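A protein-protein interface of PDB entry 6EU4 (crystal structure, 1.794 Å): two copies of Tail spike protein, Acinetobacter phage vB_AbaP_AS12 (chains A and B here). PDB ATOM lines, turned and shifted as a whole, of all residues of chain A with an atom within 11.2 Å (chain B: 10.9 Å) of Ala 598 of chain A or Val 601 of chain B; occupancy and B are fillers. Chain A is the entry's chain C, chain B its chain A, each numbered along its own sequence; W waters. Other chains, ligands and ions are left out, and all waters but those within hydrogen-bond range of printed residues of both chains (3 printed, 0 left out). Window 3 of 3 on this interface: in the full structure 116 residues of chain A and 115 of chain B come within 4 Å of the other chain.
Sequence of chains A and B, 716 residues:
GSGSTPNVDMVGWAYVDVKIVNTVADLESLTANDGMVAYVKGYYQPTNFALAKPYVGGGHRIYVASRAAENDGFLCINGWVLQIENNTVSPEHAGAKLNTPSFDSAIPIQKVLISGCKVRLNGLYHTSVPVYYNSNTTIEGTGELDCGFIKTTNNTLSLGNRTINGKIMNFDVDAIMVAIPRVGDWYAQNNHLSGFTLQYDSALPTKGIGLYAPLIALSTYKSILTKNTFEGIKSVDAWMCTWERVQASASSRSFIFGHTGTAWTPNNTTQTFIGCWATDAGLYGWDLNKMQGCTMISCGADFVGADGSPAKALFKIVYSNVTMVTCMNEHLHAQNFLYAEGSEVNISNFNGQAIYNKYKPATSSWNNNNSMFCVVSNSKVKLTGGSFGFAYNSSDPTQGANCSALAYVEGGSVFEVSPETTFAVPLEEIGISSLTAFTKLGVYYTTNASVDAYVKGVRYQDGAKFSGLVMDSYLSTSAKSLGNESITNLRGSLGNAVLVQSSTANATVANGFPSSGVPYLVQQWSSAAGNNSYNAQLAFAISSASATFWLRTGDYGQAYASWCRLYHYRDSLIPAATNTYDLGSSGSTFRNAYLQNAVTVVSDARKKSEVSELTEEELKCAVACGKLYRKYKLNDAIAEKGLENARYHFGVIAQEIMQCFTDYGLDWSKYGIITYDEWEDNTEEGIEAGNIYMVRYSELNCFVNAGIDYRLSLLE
Among the printed residues, pairs that only touch across the chains: Ala 593 of chain A with Leu 595 of chain B, Ala 593 of chain A with Val 599 of chain B, Tyr 594 of chain A with Thr 600 of chain B, Leu 595 of chain A with Val 599 of chain B, Leu 595 of chain A with Val 601 of chain B, Gln 596 of chain A with Asn 579 of chain B, Gln 596 of chain A with Val 601 of chain B, Asn 597 of chain A with Val 601 of chain B, Ala 598 of chain A with Val 601 of chain B and Val 599 of chain A with Val 599 of chain B.
Printed residues of chain B within 4 Å of Ala 598 of chain A: Val 601 (3.8 Å). Val 601 of chain B touches four residues of chain A. Asn 597 of chain A touches just one residue of chain B: Val 601. Val 599 of chain A touches one residue of chain B. Val 599 of chain B touches three residues of chain A. Of chain A, only Ala 593 (2.8 Å), Tyr 594 (3.4 Å) and Leu 595 (3.0 Å) come within 4 Å of Thr 600 of chain B. Val 602 of chain B touches just one residue of chain A: Leu 595 (2.7 Å). Printed residues of chain B within 4 Å of Asn 592 of chain A: Asn 597 (3.4 Å). Printed residues of chain A within 4 Å of Leu 595 of chain B: Ala 593. Val 602 of chain A touches none of the printed residues of chain B. Ala 598 of chain B touches none of the printed residues of chain A. The nearest residue of chain B that does not touch Ala 598 of chain A is Val 599 of chain B (5.8 Å).
Of the 11 printed residues of chain A, 8 touch a printed residue of chain B. Hydrophobic or aromatic side chains of chain A that line the printed part of chain B: Ala 593, Tyr 594, Leu 595 and Val 599. Of the 12 printed residues of chain B, 7 touch a printed residue of chain A. Hydrophobic or aromatic side chains of chain B within 4 Å of the printed part of chain A: Leu 595, Val 599, Val 601 and Val 602. Among the printed residues, 14 pairs touch across the chains.
Leu 595 of chain A touches Val 599 of chain B, but with the chains exchanged Val 599 of chain A does not touch Leu 595 of chain B (6.6 Å). Leu 595 of chain A touches Val 601 of chain B, but with the chains exchanged Val 601 of chain A does not touch Leu 595 of chain B (11.2 Å). Asn 597 of chain A touches Val 601 of chain B, but with the chains exchanged Val 601 of chain A does not touch Asn 597 of chain B (13.2 Å). Val 599 of chain A touches its own counterpart, Val 599 of chain B.
OD1 of Asn 592 of chain A lies close to OD1 of Asn 597 of chain B, at 3.5 Å. The backbone carbonyl oxygen of Ala 593 of chain A lies within hydrogen-bond range of the backbone NH of Thr 600 of chain B (2.8 Å). The backbone NH of Val 602 of chain B is in hydrogen-bond range of the backbone carbonyl oxygen of Leu 595 of chain A (2.7 Å). The backbone NH (N) of Leu 595 of chain A is in hydrogen-bond range of the backbone carbonyl oxygen (O) of Thr 600 of chain B, 3.0 Å away.
Water W2 lies within hydrogen-bond range of the backbone carbonyl oxygen (O) of Ala 598 of chain B (2.6 Å), the side-chain amide oxygen (OD1) of Asn 592 of chain A (2.7 Å), the side-chain hydroxyl (OG1) of Thr 600 of chain B (2.9 Å) and the backbone NH (N) of Ala 593 of chain A (3.1 Å). Water W1 bridges the side-chain hydroxyl (OG1) of Thr 578 of chain B (2.6 Å) and the side-chain amide oxygen (OE1) of Gln 596 of chain A (2.7 Å). Water W3 lies within hydrogen-bond range of the side-chain amide oxygen (OD1) of Asn 579 of chain B (2.8 Å) and the side-chain amide nitrogen (ND2) of Asn 597 of chain A (3.0 Å).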
ATOM      1  N   ASN A 592       0.647   2.325 -15.673  1.00  0.00           N
ATOM      2  CA  ASN A 592       0.623   3.772 -15.851  1.00  0.00           C
ATOM      3  C   ASN A 592      -0.489   4.371 -15.005  1.00  0.00           C
ATOM      4  O   ASN A 592      -1.400   3.674 -14.558  1.00  0.00           O
ATOM      5  CB  ASN A 592       0.398   4.160 -17.313  1.00  0.00           C
ATOM      6  CG  ASN A 592       1.640   3.992 -18.155  1.00  0.00           C
ATOM      7  OD1 ASN A 592       2.675   4.602 -17.884  1.00  0.00           O
ATOM      8  ND2 ASN A 592       1.548   3.150 -19.179  1.00  0.00           N
ATOM      9  N   ALA A 593      -0.412   5.682 -14.802  1.00  0.00           N
ATOM     10  CA  ALA A 593      -1.483   6.429 -14.155  1.00  0.00           C
ATOM     11  C   ALA A 593      -1.724   7.692 -14.964  1.00  0.00           C
ATOM     12  O   ALA A 593      -0.775   8.413 -15.287  1.00  0.00           O
ATOM     13  CB  ALA A 593      -1.144   6.780 -12.703  1.00  0.00           C
ATOM     14  N   TYR A 594      -2.982   7.946 -15.303  1.00  0.00           N
ATOM     15  CA  TYR A 594      -3.367   9.089 -16.128  1.00  0.00           C
ATOM     16  C   TYR A 594      -4.151  10.062 -15.259  1.00  0.00           C
ATOM     17  O   TYR A 594      -5.295   9.780 -14.883  1.00  0.00           O
ATOM     18  CB  TYR A 594      -4.188   8.628 -17.333  1.00  0.00           C
ATOM     19  CG  TYR A 594      -3.411   7.724 -18.261  1.00  0.00           C
ATOM     20  CD1 TYR A 594      -3.349   6.359 -18.042  1.00  0.00           C
ATOM     21  CD2 TYR A 594      -2.713   8.248 -19.346  1.00  0.00           C
ATOM     22  CE1 TYR A 594      -2.626   5.526 -18.884  1.00  0.00           C
ATOM     23  CE2 TYR A 594      -1.988   7.426 -20.194  1.00  0.00           C
ATOM     24  CZ  TYR A 594      -1.948   6.067 -19.961  1.00  0.00           C
ATOM     25  OH  TYR A 594      -1.225   5.261 -20.805  1.00  0.00           O
ATOM     26  N   LEU A 595      -3.533  11.196 -14.939  1.00  0.00           N
ATOM     27  CA  LEU A 595      -4.156  12.229 -14.130  1.00  0.00           C
ATOM     28  C   LEU A 595      -4.309  13.504 -14.947  1.00  0.00           C
ATOM     29  O   LEU A 595      -3.478  13.819 -15.804  1.00  0.00           O
ATOM     30  CB  LEU A 595      -3.329  12.521 -12.879  1.00  0.00           C
ATOM     31  CG  LEU A 595      -2.891  11.323 -12.030  1.00  0.00           C
ATOM     32  CD1 LEU A 595      -2.092  11.797 -10.823  1.00  0.00           C
ATOM     33  CD2 LEU A 595      -4.086  10.507 -11.578  1.00  0.00           C
ATOM     34  N   GLN A 596      -5.387  14.245 -14.676  1.00  0.00           N
ATOM     35  CA  GLN A 596      -5.528  15.560 -15.294  1.00  0.00           C
ATOM     36  C   GLN A 596      -4.534  16.551 -14.706  1.00  0.00           C
ATOM     37  O   GLN A 596      -4.054  17.449 -15.413  1.00  0.00           O
ATOM     38  CB  GLN A 596      -6.958  16.077 -15.123  1.00  0.00           C
ATOM     39  CG  GLN A 596      -7.321  17.178 -16.123  1.00  0.00           C
ATOM     40  CD  GLN A 596      -7.570  16.632 -17.523  1.00  0.00           C
ATOM     41  OE1 GLN A 596      -7.977  15.475 -17.694  1.00  0.00           O
ATOM     42  NE2 GLN A 596      -7.328  17.463 -18.532  1.00  0.00           N
ATOM     43  N   ASN A 597      -4.208  16.396 -13.425  1.00  0.00           N
ATOM     44  CA  ASN A 597      -3.298  17.288 -12.723  1.00  0.00           C
ATOM     45  C   ASN A 597      -2.197  16.482 -12.055  1.00  0.00           C
ATOM     46  O   ASN A 597      -2.362  15.296 -11.759  1.00  0.00           O
ATOM     47  CB  ASN A 597      -4.037  18.114 -11.669  1.00  0.00           C
ATOM     48  CG  ASN A 597      -5.190  18.880 -12.258  1.00  0.00           C
ATOM     49  OD1 ASN A 597      -4.983  19.860 -12.960  1.00  0.00           O
ATOM     50  ND2 ASN A 597      -6.403  18.428 -12.000  1.00  0.00           N
ATOM     51  N   ALA A 598      -1.069  17.150 -11.815  1.00  0.00           N
ATOM     52  CA  ALA A 598       0.042  16.514 -11.121  1.00  0.00           C
ATOM     53  C   ALA A 598      -0.402  16.041  -9.745  1.00  0.00           C
ATOM     54  O   ALA A 598      -1.281  16.637  -9.112  1.00  0.00           O
ATOM     55  CB  ALA A 598       1.217  17.481 -10.988  1.00  0.00           C
ATOM     56  N   VAL A 599       0.208  14.941  -9.292  1.00  0.00           N
ATOM     57  CA  VAL A 599      -0.091  14.396  -7.973  1.00  0.00           C
ATOM     58  C   VAL A 599       0.032  15.484  -6.912  1.00  0.00           C
ATOM     59  O   VAL A 599       0.959  16.297  -6.934  1.00  0.00           O
ATOM     60  CB  VAL A 599       0.856  13.219  -7.669  1.00  0.00           C
ATOM     61  CG1 VAL A 599       0.749  12.786  -6.206  1.00  0.00           C
ATOM     62  CG2 VAL A 599       0.552  12.047  -8.584  1.00  0.00           C
ATOM     63  N   THR A 600      -0.893  15.481  -5.961  1.00  0.00           N
ATOM     64  CA  THR A 600      -0.834  16.372  -4.807  1.00  0.00           C
ATOM     65  C   THR A 600      -0.200  15.597  -3.660  1.00  0.00           C
ATOM     66  O   THR A 600      -0.805  14.658  -3.138  1.00  0.00           O
ATOM     67  CB  THR A 600      -2.228  16.873  -4.423  1.00  0.00           C
ATOM     68  OG1 THR A 600      -2.806  17.588  -5.521  1.00  0.00           O
ATOM     69  CG2 THR A 600      -2.166  17.788  -3.213  1.00  0.00           C
ATOM     70  N   VAL A 601       1.024  15.973  -3.281  1.00  0.00           N
ATOM     71  CA  VAL A 601       1.733  15.300  -2.195  1.00  0.00           C
ATOM     72  C   VAL A 601       1.466  16.073  -0.907  1.00  0.00           C
ATOM     73  O   VAL A 601       1.943  17.195  -0.730  1.00  0.00           O
ATOM     74  CB  VAL A 601       3.236  15.189  -2.474  1.00  0.00           C
ATOM     75  CG1 VAL A 601       3.936  14.465  -1.314  1.00  0.00           C
ATOM     76  CG2 VAL A 601       3.482  14.464  -3.795  1.00  0.00           C
ATOM     77  N   VAL A 602       0.732  15.457   0.008  1.00  0.00           N
ATOM     78  CA  VAL A 602       0.249  16.143   1.206  1.00  0.00           C
ATOM     79  C   VAL A 602       1.334  16.224   2.286  1.00  0.00           C
ATOM     80  O   VAL A 602       2.072  15.251   2.497  1.00  0.00           O
ATOM     81  CB  VAL A 602      -1.012  15.437   1.725  1.00  0.00           C
ATOM     82  CG1 VAL A 602      -1.467  16.002   3.061  1.00  0.00           C
ATOM     83  CG2 VAL A 602      -2.119  15.547   0.689  1.00  0.00           C
ATOM     84  N   THR B 578     -14.140  11.487 -17.489  1.00  0.00           N
ATOM     85  CA  THR B 578     -12.796  12.015 -17.327  1.00  0.00           C
ATOM     86  C   THR B 578     -12.790  13.241 -16.418  1.00  0.00           C
ATOM     87  O   THR B 578     -13.788  13.958 -16.296  1.00  0.00           O
ATOM     88  CB  THR B 578     -12.196  12.367 -18.695  1.00  0.00           C
ATOM     89  OG1 THR B 578     -10.777  12.517 -18.573  1.00  0.00           O
ATOM     90  CG2 THR B 578     -12.813  13.658 -19.277  1.00  0.00           C
ATOM     91  N   ASN B 579     -11.650  13.460 -15.756  1.00  0.00           N
ATOM     92  CA  ASN B 579     -11.400  14.702 -15.012  1.00  0.00           C
ATOM     93  C   ASN B 579     -12.534  14.999 -14.026  1.00  0.00           C
ATOM     94  O   ASN B 579     -12.955  16.148 -13.841  1.00  0.00           O
ATOM     95  CB  ASN B 579     -11.196  15.867 -15.980  1.00  0.00           C
ATOM     96  CG  ASN B 579     -10.647  17.093 -15.302  1.00  0.00           C
ATOM     97  OD1 ASN B 579      -9.956  16.997 -14.289  1.00  0.00           O
ATOM     98  ND2 ASN B 579     -10.937  18.265 -15.869  1.00  0.00           N
ATOM     99  N   TYR B 581     -13.238  12.273 -11.056  1.00  0.00           N
ATOM    100  CA  TYR B 581     -13.082  11.511  -9.827  1.00  0.00           C
ATOM    101  C   TYR B 581     -11.628  11.516  -9.372  1.00  0.00           C
ATOM    102  O   TYR B 581     -10.699  11.601 -10.183  1.00  0.00           O
ATOM    103  CB  TYR B 581     -13.576  10.075 -10.028  1.00  0.00           C
ATOM    104  CG  TYR B 581     -15.035  10.027 -10.454  1.00  0.00           C
ATOM    105  CD1 TYR B 581     -16.051  10.354  -9.561  1.00  0.00           C
ATOM    106  CD2 TYR B 581     -15.392   9.686 -11.753  1.00  0.00           C
ATOM    107  CE1 TYR B 581     -17.395  10.324  -9.942  1.00  0.00           C
ATOM    108  CE2 TYR B 581     -16.737   9.652 -12.147  1.00  0.00           C
ATOM    109  CZ  TYR B 581     -17.727   9.980 -11.242  1.00  0.00           C
ATOM    110  OH  TYR B 581     -19.054   9.952 -11.630  1.00  0.00           O
ATOM    111  N   ASP B 582     -11.441  11.441  -8.056  1.00  0.00           N
ATOM    112  CA  ASP B 582     -10.129  11.576  -7.445  1.00  0.00           C
ATOM    113  C   ASP B 582      -9.660  10.249  -6.867  1.00  0.00           C
ATOM    114  O   ASP B 582     -10.471   9.399  -6.484  1.00  0.00           O
ATOM    115  CB  ASP B 582     -10.134  12.598  -6.305  1.00  0.00           C
ATOM    116  CG  ASP B 582     -10.369  14.025  -6.763  1.00  0.00           C
ATOM    117  OD1 ASP B 582     -10.076  14.360  -7.935  1.00  0.00           O
ATOM    118  OD2 ASP B 582     -10.814  14.832  -5.904  1.00  0.00           O
ATOM    119  N   LEU B 583      -8.335  10.095  -6.817  1.00  0.00           N
ATOM    120  CA  LEU B 583      -7.671   9.087  -5.995  1.00  0.00           C
ATOM    121  C   LEU B 583      -7.302   9.764  -4.682  1.00  0.00           C
ATOM    122  O   LEU B 583      -6.396  10.604  -4.639  1.00  0.00           O
ATOM    123  CB  LEU B 583      -6.432   8.539  -6.698  1.00  0.00           C
ATOM    124  CG  LEU B 583      -6.723   7.852  -8.026  1.00  0.00           C
ATOM    125  CD1 LEU B 583      -5.460   7.676  -8.824  1.00  0.00           C
ATOM    126  CD2 LEU B 583      -7.416   6.527  -7.802  1.00  0.00           C
ATOM    127  N   LEU B 595       4.120   2.709  -9.162  1.00  0.00           N
ATOM    128  CA  LEU B 595       3.925   2.681 -10.600  1.00  0.00           C
ATOM    129  C   LEU B 595       5.196   2.190 -11.274  1.00  0.00           C
ATOM    130  O   LEU B 595       6.309   2.467 -10.814  1.00  0.00           O
ATOM    131  CB  LEU B 595       3.571   4.071 -11.150  1.00  0.00           C
ATOM    132  CG  LEU B 595       2.447   4.819 -10.429  1.00  0.00           C
ATOM    133  CD1 LEU B 595       2.175   6.146 -11.127  1.00  0.00           C
ATOM    134  CD2 LEU B 595       1.175   3.987 -10.333  1.00  0.00           C
ATOM    135  N   ASN B 597       5.901   3.255 -14.267  1.00  0.00           N
ATOM    136  CA  ASN B 597       6.319   4.440 -15.000  1.00  0.00           C
ATOM    137  C   ASN B 597       5.839   5.693 -14.284  1.00  0.00           C
ATOM    138  O   ASN B 597       4.930   5.654 -13.454  1.00  0.00           O
ATOM    139  CB  ASN B 597       5.775   4.427 -16.429  1.00  0.00           C
ATOM    140  CG  ASN B 597       6.042   3.125 -17.137  1.00  0.00           C
ATOM    141  OD1 ASN B 597       5.170   2.256 -17.238  1.00  0.00           O
ATOM    142  ND2 ASN B 597       7.256   2.967 -17.616  1.00  0.00           N
ATOM    143  N   ALA B 598       6.456   6.820 -14.628  1.00  0.00           N
ATOM    144  CA  ALA B 598       6.032   8.094 -14.070  1.00  0.00           C
ATOM    145  C   ALA B 598       4.592   8.404 -14.466  1.00  0.00           C
ATOM    146  O   ALA B 598       4.116   8.018 -15.541  1.00  0.00           O
ATOM    147  CB  ALA B 598       6.965   9.213 -14.542  1.00  0.00           C
ATOM    148  N   VAL B 599       3.891   9.098 -13.562  1.00  0.00           N
ATOM    149  CA  VAL B 599       2.531   9.549 -13.826  1.00  0.00           C
ATOM    150  C   VAL B 599       2.470  10.305 -15.140  1.00  0.00           C
ATOM    151  O   VAL B 599       3.329  11.142 -15.435  1.00  0.00           O
ATOM    152  CB  VAL B 599       2.030  10.438 -12.676  1.00  0.00           C
ATOM    153  CG1 VAL B 599       0.720  11.126 -13.064  1.00  0.00           C
ATOM    154  CG2 VAL B 599       1.839   9.614 -11.399  1.00  0.00           C
ATOM    155  N   THR B 600       1.429  10.027 -15.924  1.00  0.00           N
ATOM    156  CA  THR B 600       1.143  10.768 -17.147  1.00  0.00           C
ATOM    157  C   THR B 600       0.138  11.865 -16.811  1.00  0.00           C
ATOM    158  O   THR B 600      -1.029  11.579 -16.518  1.00  0.00           O
ATOM    159  CB  THR B 600       0.596   9.836 -18.226  1.00  0.00           C
ATOM    160  OG1 THR B 600       1.538   8.781 -18.466  1.00  0.00           O
ATOM    161  CG2 THR B 600       0.325  10.593 -19.525  1.00  0.00           C
ATOM    162  N   VAL B 601       0.587  13.115 -16.852  1.00  0.00           N
ATOM    163  CA  VAL B 601      -0.268  14.254 -16.536  1.00  0.00           C
ATOM    164  C   VAL B 601      -0.864  14.759 -17.841  1.00  0.00           C
ATOM    165  O   VAL B 601      -0.171  15.377 -18.658  1.00  0.00           O
ATOM    166  CB  VAL B 601       0.503  15.359 -15.811  1.00  0.00           C
ATOM    167  CG1 VAL B 601      -0.423  16.554 -15.531  1.00  0.00           C
ATOM    168  CG2 VAL B 601       1.096  14.815 -14.515  1.00  0.00           C
ATOM    169  N   VAL B 602      -2.157  14.520 -18.018  1.00  0.00           N
ATOM    170  CA  VAL B 602      -2.848  14.836 -19.253  1.00  0.00           C
ATOM    171  C   VAL B 602      -3.225  16.305 -19.285  1.00  0.00           C
ATOM    172  O   VAL B 602      -3.280  16.892 -20.359  1.00  0.00           O
ATOM    173  CB  VAL B 602      -4.091  13.948 -19.416  1.00  0.00           C
ATOM    174  CG1 VAL B 602      -4.843  14.294 -20.685  1.00  0.00           C
ATOM    175  CG2 VAL B 602      -3.688  12.469 -19.405  1.00  0.00           C
HETATM  176  O   HOH W   1      -9.443  14.480 -19.699  1.00  0.00           O
HETATM  177  O   HOH W   2       1.969   6.808 -16.406  1.00  0.00           O
HETATM  178  O   HOH W   3      -8.997  19.338 -13.089  1.00  0.00           O
